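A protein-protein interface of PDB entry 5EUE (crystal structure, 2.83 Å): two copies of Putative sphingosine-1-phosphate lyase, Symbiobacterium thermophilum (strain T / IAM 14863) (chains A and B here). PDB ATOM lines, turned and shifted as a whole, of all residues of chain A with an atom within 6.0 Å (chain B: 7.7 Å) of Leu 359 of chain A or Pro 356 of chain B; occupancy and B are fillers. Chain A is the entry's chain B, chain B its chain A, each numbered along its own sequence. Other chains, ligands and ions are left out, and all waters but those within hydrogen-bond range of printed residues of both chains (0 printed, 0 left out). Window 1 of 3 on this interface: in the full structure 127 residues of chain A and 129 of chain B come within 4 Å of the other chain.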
ATOM      1  N   TYR A 120      21.513  23.773 -12.094  1.00  0.00           N
ATOM      2  CA  TYR A 120      20.499  22.965 -11.412  1.00  0.00           C
ATOM      3  C   TYR A 120      19.177  23.177 -12.114  1.00  0.00           C
ATOM      4  O   TYR A 120      18.622  22.233 -12.665  1.00  0.00           O
ATOM      5  CB  TYR A 120      20.372  23.290  -9.896  1.00  0.00           C
ATOM      6  CG  TYR A 120      19.306  22.444  -9.220  1.00  0.00           C
ATOM      7  CD1 TYR A 120      19.624  21.215  -8.648  1.00  0.00           C
ATOM      8  CD2 TYR A 120      17.959  22.821  -9.253  1.00  0.00           C
ATOM      9  CE1 TYR A 120      18.636  20.373  -8.142  1.00  0.00           C
ATOM     10  CE2 TYR A 120      16.962  21.985  -8.747  1.00  0.00           C
ATOM     11  CZ  TYR A 120      17.308  20.764  -8.188  1.00  0.00           C
ATOM     12  OH  TYR A 120      16.354  19.936  -7.659  1.00  0.00           O
ATOM     13  N   SER A 167      26.049   9.477  -4.708  1.00  0.00           N
ATOM     14  CA  SER A 167      25.438  10.510  -3.857  1.00  0.00           C
ATOM     15  C   SER A 167      26.409  11.133  -2.842  1.00  0.00           C
ATOM     16  O   SER A 167      26.080  12.140  -2.196  1.00  0.00           O
ATOM     17  CB  SER A 167      24.270   9.901  -3.104  1.00  0.00           C
ATOM     18  OG  SER A 167      24.726   8.768  -2.385  1.00  0.00           O
ATOM     19  N   ALA A 317      28.099  20.897  -6.718  1.00  0.00           N
ATOM     20  CA  ALA A 317      27.082  21.028  -5.672  1.00  0.00           C
ATOM     21  C   ALA A 317      26.929  19.706  -4.884  1.00  0.00           C
ATOM     22  O   ALA A 317      27.152  18.631  -5.446  1.00  0.00           O
ATOM     23  CB  ALA A 317      25.761  21.444  -6.291  1.00  0.00           C
ATOM     24  N   LYS A 318      26.571  19.790  -3.586  1.00  0.00           N
ATOM     25  CA  LYS A 318      26.385  18.623  -2.712  1.00  0.00           C
ATOM     26  C   LYS A 318      25.537  17.524  -3.352  1.00  0.00           C
ATOM     27  O   LYS A 318      24.586  17.805  -4.084  1.00  0.00           O
ATOM     28  CB  LYS A 318      25.815  19.002  -1.316  1.00  0.00           C
ATOM     29  CG  LYS A 318      26.814  19.597  -0.318  1.00  0.00           C
ATOM     30  CD  LYS A 318      28.153  18.802  -0.228  1.00  0.00           C
ATOM     31  CE  LYS A 318      29.361  19.643   0.124  1.00  0.00           C
ATOM     32  NZ  LYS A 318      29.618  19.648   1.596  1.00  0.00           N
ATOM     33  N   GLY A 319      25.891  16.282  -3.064  1.00  0.00           N
ATOM     34  CA  GLY A 319      25.153  15.130  -3.551  1.00  0.00           C
ATOM     35  C   GLY A 319      25.797  14.381  -4.686  1.00  0.00           C
ATOM     36  O   GLY A 319      25.084  13.685  -5.403  1.00  0.00           O
ATOM     37  N   THR A 320      27.135  14.522  -4.871  1.00  0.00           N
ATOM     38  CA  THR A 320      27.915  13.824  -5.905  1.00  0.00           C
ATOM     39  C   THR A 320      29.312  13.399  -5.467  1.00  0.00           C
ATOM     40  O   THR A 320      30.026  14.124  -4.771  1.00  0.00           O
ATOM     41  CB  THR A 320      28.008  14.573  -7.237  1.00  0.00           C
ATOM     42  OG1 THR A 320      28.337  15.948  -7.014  1.00  0.00           O
ATOM     43  CG2 THR A 320      26.761  14.404  -8.099  1.00  0.00           C
ATOM     44  N   PRO A 356      18.800  12.550  -8.259  1.00  0.00           N
ATOM     45  CA  PRO A 356      18.664  13.928  -8.755  1.00  0.00           C
ATOM     46  C   PRO A 356      19.743  14.141  -9.813  1.00  0.00           C
ATOM     47  O   PRO A 356      20.909  14.371  -9.474  1.00  0.00           O
ATOM     48  CB  PRO A 356      18.918  14.791  -7.516  1.00  0.00           C
ATOM     49  CG  PRO A 356      19.423  13.853  -6.460  1.00  0.00           C
ATOM     50  CD  PRO A 356      19.609  12.509  -7.027  1.00  0.00           C
ATOM     51  N   GLY A 357      19.368  13.986 -11.078  1.00  0.00           N
ATOM     52  CA  GLY A 357      20.294  14.158 -12.191  1.00  0.00           C
ATOM     53  C   GLY A 357      20.937  15.531 -12.243  1.00  0.00           C
ATOM     54  O   GLY A 357      22.087  15.660 -12.670  1.00  0.00           O
ATOM     55  N   ALA A 358      20.211  16.554 -11.773  1.00  0.00           N
ATOM     56  CA  ALA A 358      20.680  17.927 -11.720  1.00  0.00           C
ATOM     57  C   ALA A 358      21.988  18.073 -10.947  1.00  0.00           C
ATOM     58  O   ALA A 358      22.799  18.931 -11.295  1.00  0.00           O
ATOM     59  CB  ALA A 358      19.617  18.822 -11.124  1.00  0.00           C
ATOM     60  N   LEU A 359      22.221  17.218  -9.938  1.00  0.00           N
ATOM     61  CA  LEU A 359      23.460  17.268  -9.149  1.00  0.00           C
ATOM     62  C   LEU A 359      24.682  16.785  -9.955  1.00  0.00           C
ATOM     63  O   LEU A 359      25.767  17.346  -9.800  1.00  0.00           O
ATOM     64  CB  LEU A 359      23.320  16.551  -7.797  1.00  0.00           C
ATOM     65  CG  LEU A 359      22.090  16.930  -6.952  1.00  0.00           C
ATOM     66  CD1 LEU A 359      22.067  16.150  -5.657  1.00  0.00           C
ATOM     67  CD2 LEU A 359      22.022  18.438  -6.681  1.00  0.00           C
ATOM     68  N   SER A 360      24.486  15.806 -10.860  1.00  0.00           N
ATOM     69  CA  SER A 360      25.548  15.333 -11.751  1.00  0.00           C
ATOM     70  C   SER A 360      25.937  16.450 -12.744  1.00  0.00           C
ATOM     71  O   SER A 360      27.135  16.685 -12.942  1.00  0.00           O
ATOM     72  CB  SER A 360      25.111  14.090 -12.507  1.00  0.00           C
ATOM     73  OG  SER A 360      25.124  12.987 -11.623  1.00  0.00           O
ATOM     74  N   ALA A 361      24.942  17.162 -13.326  1.00  0.00           N
ATOM     75  CA  ALA A 361      25.222  18.289 -14.221  1.00  0.00           C
ATOM     76  C   ALA A 361      26.104  19.379 -13.521  1.00  0.00           C
ATOM     77  O   ALA A 361      26.963  19.966 -14.189  1.00  0.00           O
ATOM     78  CB  ALA A 361      23.928  18.906 -14.728  1.00  0.00           C
ATOM     79  N   THR A 362      25.927  19.600 -12.180  1.00  0.00           N
ATOM     80  CA  THR A 362      26.677  20.612 -11.441  1.00  0.00           C
ATOM     81  C   THR A 362      28.122  20.219 -11.312  1.00  0.00           C
ATOM     82  O   THR A 362      28.986  21.096 -11.373  1.00  0.00           O
ATOM     83  CB  THR A 362      26.042  20.978 -10.094  1.00  0.00           C
ATOM     84  OG1 THR A 362      26.173  19.904  -9.163  1.00  0.00           O
ATOM     85  CG2 THR A 362      24.591  21.444 -10.217  1.00  0.00           C
ATOM     86  N   ALA A 363      28.402  18.909 -11.151  1.00  0.00           N
ATOM     87  CA  ALA A 363      29.774  18.421 -11.061  1.00  0.00           C
ATOM     88  C   ALA A 363      30.443  18.550 -12.441  1.00  0.00           C
ATOM     89  O   ALA A 363      31.576  18.992 -12.541  1.00  0.00           O
ATOM     90  CB  ALA A 363      29.789  16.980 -10.594  1.00  0.00           C
ATOM     91  N   TRP A 364      29.719  18.227 -13.500  1.00  0.00           N
ATOM     92  CA  TRP A 364      30.201  18.356 -14.863  1.00  0.00           C
ATOM     93  C   TRP A 364      30.474  19.847 -15.191  1.00  0.00           C
ATOM     94  O   TRP A 364      31.534  20.171 -15.724  1.00  0.00           O
ATOM     95  CB  TRP A 364      29.170  17.721 -15.792  1.00  0.00           C
ATOM     96  CG  TRP A 364      29.534  17.725 -17.235  1.00  0.00           C
ATOM     97  CD1 TRP A 364      30.292  16.805 -17.891  1.00  0.00           C
ATOM     98  CD2 TRP A 364      29.045  18.629 -18.231  1.00  0.00           C
ATOM     99  NE1 TRP A 364      30.292  17.066 -19.237  1.00  0.00           N
ATOM    100  CE2 TRP A 364      29.513  18.167 -19.480  1.00  0.00           C
ATOM    101  CE3 TRP A 364      28.192  19.751 -18.198  1.00  0.00           C
ATOM    102  CZ2 TRP A 364      29.221  18.829 -20.682  1.00  0.00           C
ATOM    103  CZ3 TRP A 364      27.908  20.408 -19.389  1.00  0.00           C
ATOM    104  CH2 TRP A 364      28.447  19.965 -20.609  1.00  0.00           C
ATOM    105  N   TYR B 120      15.673  25.514  -4.046  1.00  0.00           N
ATOM    106  CA  TYR B 120      16.960  24.862  -4.177  1.00  0.00           C
ATOM    107  C   TYR B 120      18.090  25.875  -4.038  1.00  0.00           C
ATOM    108  O   TYR B 120      18.988  25.652  -3.246  1.00  0.00           O
ATOM    109  CB  TYR B 120      17.078  24.125  -5.527  1.00  0.00           C
ATOM    110  CG  TYR B 120      18.464  23.575  -5.714  1.00  0.00           C
ATOM    111  CD1 TYR B 120      18.812  22.334  -5.199  1.00  0.00           C
ATOM    112  CD2 TYR B 120      19.481  24.359  -6.259  1.00  0.00           C
ATOM    113  CE1 TYR B 120      20.126  21.867  -5.255  1.00  0.00           C
ATOM    114  CE2 TYR B 120      20.799  23.903  -6.318  1.00  0.00           C
ATOM    115  CZ  TYR B 120      21.115  22.655  -5.811  1.00  0.00           C
ATOM    116  OH  TYR B 120      22.396  22.181  -5.845  1.00  0.00           O
ATOM    117  N   GLN B 123      18.822  27.380  -0.531  1.00  0.00           N
ATOM    118  CA  GLN B 123      19.364  26.333   0.355  1.00  0.00           C
ATOM    119  C   GLN B 123      20.432  25.416  -0.270  1.00  0.00           C
ATOM    120  O   GLN B 123      20.710  24.372   0.312  1.00  0.00           O
ATOM    121  CB  GLN B 123      18.201  25.449   0.848  1.00  0.00           C
ATOM    122  CG  GLN B 123      17.335  26.075   1.929  1.00  0.00           C
ATOM    123  CD  GLN B 123      18.012  26.144   3.275  1.00  0.00           C
ATOM    124  OE1 GLN B 123      18.256  25.120   3.928  1.00  0.00           O
ATOM    125  NE2 GLN B 123      18.319  27.363   3.719  1.00  0.00           N
ATOM    126  N   SER B 124      21.019  25.784  -1.432  1.00  0.00           N
ATOM    127  CA  SER B 124      21.979  24.966  -2.198  1.00  0.00           C
ATOM    128  C   SER B 124      23.244  24.533  -1.441  1.00  0.00           C
ATOM    129  O   SER B 124      23.815  23.485  -1.766  1.00  0.00           O
ATOM    130  CB  SER B 124      22.369  25.659  -3.498  1.00  0.00           C
ATOM    131  OG  SER B 124      22.998  26.912  -3.283  1.00  0.00           O
ATOM    132  N   GLN B 125      23.674  25.319  -0.436  1.00  0.00           N
ATOM    133  CA  GLN B 125      24.879  25.011   0.348  1.00  0.00           C
ATOM    134  C   GLN B 125      24.649  24.063   1.529  1.00  0.00           C
ATOM    135  O   GLN B 125      25.619  23.458   1.992  1.00  0.00           O
ATOM    136  CB  GLN B 125      25.588  26.302   0.821  1.00  0.00           C
ATOM    137  CG  GLN B 125      26.027  27.230  -0.312  1.00  0.00           C
ATOM    138  CD  GLN B 125      26.991  26.554  -1.248  1.00  0.00           C
ATOM    139  OE1 GLN B 125      28.152  26.280  -0.895  1.00  0.00           O
ATOM    140  NE2 GLN B 125      26.513  26.265  -2.464  1.00  0.00           N
ATOM    141  N   SER B 126      23.386  23.918   2.005  1.00  0.00           N
ATOM    142  CA  SER B 126      23.008  23.079   3.155  1.00  0.00           C
ATOM    143  C   SER B 126      23.350  21.584   3.043  1.00  0.00           C
ATOM    144  O   SER B 126      23.198  20.968   1.983  1.00  0.00           O
ATOM    145  CB  SER B 126      21.533  23.237   3.484  1.00  0.00           C
ATOM    146  OG  SER B 126      20.755  22.687   2.438  1.00  0.00           O
ATOM    147  N   ASN B 127      23.788  21.020   4.169  1.00  0.00           N
ATOM    148  CA  ASN B 127      24.170  19.625   4.333  1.00  0.00           C
ATOM    149  C   ASN B 127      23.716  19.170   5.741  1.00  0.00           C
ATOM    150  O   ASN B 127      24.277  19.647   6.734  1.00  0.00           O
ATOM    151  CB  ASN B 127      25.699  19.475   4.141  1.00  0.00           C
ATOM    152  CG  ASN B 127      26.274  18.084   4.322  1.00  0.00           C
ATOM    153  OD1 ASN B 127      25.606  17.066   4.132  1.00  0.00           O
ATOM    154  ND2 ASN B 127      27.557  18.015   4.650  1.00  0.00           N
ATOM    155  N   PRO B 128      22.703  18.266   5.848  1.00  0.00           N
ATOM    156  CA  PRO B 128      22.210  17.825   7.173  1.00  0.00           C
ATOM    157  C   PRO B 128      23.233  17.215   8.139  1.00  0.00           C
ATOM    158  O   PRO B 128      22.928  17.146   9.334  1.00  0.00           O
ATOM    159  CB  PRO B 128      21.120  16.808   6.820  1.00  0.00           C
ATOM    160  CG  PRO B 128      20.644  17.236   5.482  1.00  0.00           C
ATOM    161  CD  PRO B 128      21.894  17.665   4.772  1.00  0.00           C
ATOM    162  N   LEU B 129      24.437  16.806   7.647  1.00  0.00           N
ATOM    163  CA  LEU B 129      25.541  16.266   8.461  1.00  0.00           C
ATOM    164  C   LEU B 129      26.064  17.336   9.462  1.00  0.00           C
ATOM    165  O   LEU B 129      26.702  16.992  10.462  1.00  0.00           O
ATOM    166  CB  LEU B 129      26.665  15.749   7.542  1.00  0.00           C
ATOM    167  CG  LEU B 129      27.795  14.942   8.187  1.00  0.00           C
ATOM    168  CD1 LEU B 129      27.412  13.479   8.366  1.00  0.00           C
ATOM    169  CD2 LEU B 129      29.075  15.071   7.386  1.00  0.00           C
ATOM    170  N   THR B 137      17.494  22.940   7.822  1.00  0.00           N
ATOM    171  CA  THR B 137      17.350  21.656   7.133  1.00  0.00           C
ATOM    172  C   THR B 137      16.851  20.565   8.078  1.00  0.00           C
ATOM    173  O   THR B 137      16.066  19.714   7.659  1.00  0.00           O
ATOM    174  CB  THR B 137      18.636  21.283   6.417  1.00  0.00           C
ATOM    175  OG1 THR B 137      19.142  22.441   5.764  1.00  0.00           O
ATOM    176  CG2 THR B 137      18.427  20.187   5.391  1.00  0.00           C
ATOM    177  N   GLU B 141      13.418  18.601   7.419  1.00  0.00           N
ATOM    178  CA  GLU B 141      13.356  17.151   7.469  1.00  0.00           C
ATOM    179  C   GLU B 141      12.353  16.659   8.525  1.00  0.00           C
ATOM    180  O   GLU B 141      11.460  15.865   8.209  1.00  0.00           O
ATOM    181  CB  GLU B 141      14.745  16.562   7.712  1.00  0.00           C
ATOM    182  CG  GLU B 141      15.635  16.573   6.475  1.00  0.00           C
ATOM    183  CD  GLU B 141      16.832  15.642   6.497  1.00  0.00           C
ATOM    184  OE1 GLU B 141      17.452  15.458   5.424  1.00  0.00           O
ATOM    185  OE2 GLU B 141      17.145  15.083   7.574  1.00  0.00           O
ATOM    186  N   VAL B 165      13.958  11.455   6.514  1.00  0.00           N
ATOM    187  CA  VAL B 165      13.897  11.801   5.094  1.00  0.00           C
ATOM    188  C   VAL B 165      15.136  11.125   4.465  1.00  0.00           C
ATOM    189  O   VAL B 165      16.239  11.247   5.000  1.00  0.00           O
ATOM    190  CB  VAL B 165      13.846  13.355   4.858  1.00  0.00           C
ATOM    191  CG1 VAL B 165      13.853  13.719   3.380  1.00  0.00           C
ATOM    192  CG2 VAL B 165      12.640  13.977   5.527  1.00  0.00           C
ATOM    193  N   THR B 166      14.925  10.385   3.362  1.00  0.00           N
ATOM    194  CA  THR B 166      15.939   9.653   2.591  1.00  0.00           C
ATOM    195  C   THR B 166      16.067  10.228   1.145  1.00  0.00           C
ATOM    196  O   THR B 166      15.467  11.257   0.844  1.00  0.00           O
ATOM    197  CB  THR B 166      15.644   8.128   2.631  1.00  0.00           C
ATOM    198  OG1 THR B 166      14.680   7.772   1.638  1.00  0.00           O
ATOM    199  CG2 THR B 166      15.210   7.641   3.991  1.00  0.00           C
ATOM    200  N   SER B 167      16.832   9.551   0.257  1.00  0.00           N
ATOM    201  CA  SER B 167      17.094   9.959  -1.139  1.00  0.00           C
ATOM    202  C   SER B 167      16.043   9.505  -2.120  1.00  0.00           C
ATOM    203  O   SER B 167      15.752  10.198  -3.090  1.00  0.00           O
ATOM    204  CB  SER B 167      18.458   9.473  -1.607  1.00  0.00           C
ATOM    205  OG  SER B 167      18.548   8.060  -1.571  1.00  0.00           O
ATOM    206  N   LYS B 318      13.454  15.734  -7.452  1.00  0.00           N
ATOM    207  CA  LYS B 318      13.993  14.377  -7.325  1.00  0.00           C
ATOM    208  C   LYS B 318      15.143  14.345  -6.289  1.00  0.00           C
ATOM    209  O   LYS B 318      15.879  15.335  -6.137  1.00  0.00           O
ATOM    210  CB  LYS B 318      14.363  13.746  -8.695  1.00  0.00           C
ATOM    211  CG  LYS B 318      13.156  13.349  -9.560  1.00  0.00           C
ATOM    212  CD  LYS B 318      12.159  12.392  -8.867  1.00  0.00           C
ATOM    213  CE  LYS B 318      10.979  11.957  -9.702  1.00  0.00           C
ATOM    214  NZ  LYS B 318      11.286  10.782 -10.578  1.00  0.00           N
ATOM    215  N   GLY B 319      15.198  13.266  -5.511  1.00  0.00           N
ATOM    216  CA  GLY B 319      16.216  13.114  -4.485  1.00  0.00           C
ATOM    217  C   GLY B 319      15.700  13.051  -3.067  1.00  0.00           C
ATOM    218  O   GLY B 319      16.508  13.087  -2.128  1.00  0.00           O
ATOM    219  N   THR B 320      14.362  12.894  -2.894  1.00  0.00           N
ATOM    220  CA  THR B 320      13.728  12.790  -1.557  1.00  0.00           C
ATOM    221  C   THR B 320      12.591  11.727  -1.409  1.00  0.00           C
ATOM    222  O   THR B 320      11.757  11.535  -2.300  1.00  0.00           O
ATOM    223  CB  THR B 320      13.211  14.150  -1.044  1.00  0.00           C
ATOM    224  OG1 THR B 320      12.509  14.825  -2.082  1.00  0.00           O
ATOM    225  CG2 THR B 320      14.302  15.026  -0.500  1.00  0.00           C
ATOM    226  N   ALA B 352      23.492   7.509   3.754  1.00  0.00           N
ATOM    227  CA  ALA B 352      24.515   8.522   3.488  1.00  0.00           C
ATOM    228  C   ALA B 352      24.903   9.384   4.669  1.00  0.00           C
ATOM    229  O   ALA B 352      24.099   9.577   5.578  1.00  0.00           O
ATOM    230  CB  ALA B 352      24.045   9.420   2.360  1.00  0.00           C
ATOM    231  N   GLY B 353      26.114   9.940   4.598  1.00  0.00           N
ATOM    232  CA  GLY B 353      26.663  10.889   5.558  1.00  0.00           C
ATOM    233  C   GLY B 353      26.333  12.301   5.103  1.00  0.00           C
ATOM    234  O   GLY B 353      25.448  12.947   5.670  1.00  0.00           O
ATOM    235  N   SER B 354      27.005  12.781   4.041  1.00  0.00           N
ATOM    236  CA  SER B 354      26.708  14.101   3.468  1.00  0.00           C
ATOM    237  C   SER B 354      25.442  13.978   2.627  1.00  0.00           C
ATOM    238  O   SER B 354      25.338  13.104   1.754  1.00  0.00           O
ATOM    239  CB  SER B 354      27.878  14.649   2.655  1.00  0.00           C
ATOM    240  OG  SER B 354      28.939  15.055   3.505  1.00  0.00           O
ATOM    241  N   ARG B 355      24.456  14.800   2.953  1.00  0.00           N
ATOM    242  CA  ARG B 355      23.131  14.748   2.351  1.00  0.00           C
ATOM    243  C   ARG B 355      22.771  16.075   1.628  1.00  0.00           C
ATOM    244  O   ARG B 355      23.107  17.141   2.157  1.00  0.00           O
ATOM    245  CB  ARG B 355      22.123  14.333   3.462  1.00  0.00           C
ATOM    246  CG  ARG B 355      20.645  14.490   3.137  1.00  0.00           C
ATOM    247  CD  ARG B 355      19.812  13.240   3.403  1.00  0.00           C
ATOM    248  NE  ARG B 355      18.421  13.458   3.000  1.00  0.00           N
ATOM    249  CZ  ARG B 355      17.983  13.447   1.742  1.00  0.00           C
ATOM    250  NH1 ARG B 355      18.819  13.196   0.740  1.00  0.00           N
ATOM    251  NH2 ARG B 355      16.711  13.683   1.476  1.00  0.00           N
ATOM    252  N   PRO B 356      22.154  16.064   0.409  1.00  0.00           N
ATOM    253  CA  PRO B 356      21.814  17.338  -0.240  1.00  0.00           C
ATOM    254  C   PRO B 356      20.622  17.970   0.479  1.00  0.00           C
ATOM    255  O   PRO B 356      19.462  17.587   0.278  1.00  0.00           O
ATOM    256  CB  PRO B 356      21.514  16.941  -1.700  1.00  0.00           C
ATOM    257  CG  PRO B 356      21.763  15.478  -1.801  1.00  0.00           C
ATOM    258  CD  PRO B 356      21.690  14.928  -0.405  1.00  0.00           C
ATOM    259  N   GLY B 357      20.937  18.899   1.366  1.00  0.00           N
ATOM    260  CA  GLY B 357      19.953  19.591   2.185  1.00  0.00           C
ATOM    261  C   GLY B 357      18.953  20.396   1.397  1.00  0.00           C
ATOM    262  O   GLY B 357      17.798  20.529   1.803  1.00  0.00           O
ATOM    263  N   ALA B 358      19.391  20.957   0.277  1.00  0.00           N
ATOM    264  CA  ALA B 358      18.555  21.759  -0.610  1.00  0.00           C
ATOM    265  C   ALA B 358      17.326  20.997  -1.096  1.00  0.00           C
ATOM    266  O   ALA B 358      16.307  21.632  -1.371  1.00  0.00           O
ATOM    267  CB  ALA B 358      19.367  22.228  -1.797  1.00  0.00           C
ATOM    268  N   LEU B 359      17.423  19.648  -1.207  1.00  0.00           N
ATOM    269  CA  LEU B 359      16.340  18.792  -1.700  1.00  0.00           C
ATOM    270  C   LEU B 359      15.305  18.470  -0.626  1.00  0.00           C
ATOM    271  O   LEU B 359      14.146  18.260  -0.946  1.00  0.00           O
ATOM    272  CB  LEU B 359      16.876  17.520  -2.386  1.00  0.00           C
ATOM    273  CG  LEU B 359      17.863  17.735  -3.542  1.00  0.00           C
ATOM    274  CD1 LEU B 359      18.334  16.435  -4.089  1.00  0.00           C
ATOM    275  CD2 LEU B 359      17.241  18.495  -4.664  1.00  0.00           C
ATOM    276  N   SER B 360      15.709  18.474   0.639  1.00  0.00           N
ATOM    277  CA  SER B 360      14.804  18.294   1.765  1.00  0.00           C
ATOM    278  C   SER B 360      13.868  19.525   1.796  1.00  0.00           C
ATOM    279  O   SER B 360      12.649  19.380   1.978  1.00  0.00           O
ATOM    280  CB  SER B 360      15.598  18.184   3.064  1.00  0.00           C
ATOM    281  OG  SER B 360      16.462  17.058   3.006  1.00  0.00           O
ATOM    282  N   ALA B 361      14.455  20.723   1.544  1.00  0.00           N
ATOM    283  CA  ALA B 361      13.770  22.007   1.451  1.00  0.00           C
ATOM    284  C   ALA B 361      12.735  22.019   0.312  1.00  0.00           C
ATOM    285  O   ALA B 361      11.637  22.508   0.554  1.00  0.00           O
ATOM    286  CB  ALA B 361      14.774  23.132   1.276  1.00  0.00           C
ATOM    287  N   THR B 362      13.038  21.443  -0.887  1.00  0.00           N
ATOM    288  CA  THR B 362      12.056  21.364  -1.990  1.00  0.00           C
ATOM    289  C   THR B 362      10.882  20.463  -1.598  1.00  0.00           C
ATOM    290  O   THR B 362       9.750  20.776  -1.969  1.00  0.00           O
ATOM    291  CB  THR B 362      12.640  20.839  -3.299  1.00  0.00           C
ATOM    292  OG1 THR B 362      13.210  19.567  -3.057  1.00  0.00           O
ATOM    293  CG2 THR B 362      13.634  21.781  -3.948  1.00  0.00           C
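Hydrophobic or aromatic side chains of chain A within 4 Å of the printed part of chain B: Tyr 120, Ala 317, Pro 356 and Leu 359.
Among the printed residues, 10 pairs touch across the chains.
Among the printed residues, no Asp or Glu carboxylate lies within 4 Å of a Lys or Arg side-chain nitrogen of the other chain.
Tyr 120 of chain A touches its own counterpart, Tyr 120 of chain B.
Lys 318 of chain A touches Pro 356 of chain B, and with the chains exchanged Pro 356 of chain A touches Lys 318 of chain B.
Gly 319 of chain A touches Pro 356 of chain B, and with the chains exchanged Pro 356 of chain A touches Gly 319 of chain B.
Pro 356 of chain A touches Leu 359 of chain B, and with the chains exchanged Leu 359 of chain A touches Pro 356 of chain B.
Positions printed for both chains: 120, 167, 318, 319, 320, 356, 357, 358, 359, 360, 361 and 362.
Of the 10 pairs that touch across the chains among the printed residues, 9 have their exchanged pair printed and touching as well.
Tyr 120 of chain A touches Tyr 120 of chain B (CD1 to CE1, 3.5 Å).
Tyr 120 of chain A touches Leu 359 of chain B.
CB of Ala 317 of chain A touches OH of Tyr 120 of chain B, 3.5 Å away.
Lys 318 of chain A touches Pro 356 of chain B (O to CB, 3.98 Å).
Gly 319 of chain A touches Pro 356 of chain B.
O of Lys 318 of chain B touches CB of Pro 356 of chain A (3.4 Å).
Pro 356 of chain A touches Gly 319 of chain B (CG to CA, 3.8 Å).
Leu 359 of chain B touches Pro 356 of chain A (CD1 to CG, 3.7 Å).
CD2 of Leu 359 of chain A touches OH of Tyr 120 of chain B, 3.9 Å away.
CD1 of Leu 359 of chain A touches CG of Pro 356 of chain B, at 3.9 Å.
Printed residues of chain B within 4 Å of Lys 318 of chain A: Pro 356.
Ala 358 of chain A touches none of the printed residues of chain B.
Of chain B, only Tyr 120 and Pro 356 come within 4 Å of Leu 359 of chain A.
Of the printed residues of chain A, Tyr 120 of chain B touches Tyr 120 (3.5 Å), Ala 317 (3.5 Å) and Leu 359 (3.9 Å).
Of the printed residues of chain A, Pro 356 of chain B touches Lys 318, Gly 319 and Leu 359.
Ala 361 of chain B touches none of the printed residues of chain A.
The nearest residue of chain B that does not touch Leu 359 of chain A is Leu 359 of chain B (4.1 Å).
The nearest printed residue of chain A that does not touch Pro 356 of chain B is Pro 356 of chain A (5.5 Å).
The nearest printed residue of chain B that does not touch Pro 356 of chain A is Pro 356 of chain B (5.5 Å).
The backbone carbonyl oxygen of Leu 359 of chain B lies within hydrogen-bond range of the side-chain hydroxyl of Thr 362 of chain B.
The backbone carbonyl oxygen (O) of Ala 317 of chain A sits at hydrogen-bond distance from the side-chain hydroxyl (OG1) of Thr 320 of chain A (3.3 Å).
N of Ala 317 of chain A is in hydrogen-bond range of OG1 of Thr 362 of chain A, at 3.3 Å.
O of Leu 359 of chain A lies within hydrogen-bond range of OG1 of Thr 362 of chain A, 2.7 Å away.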
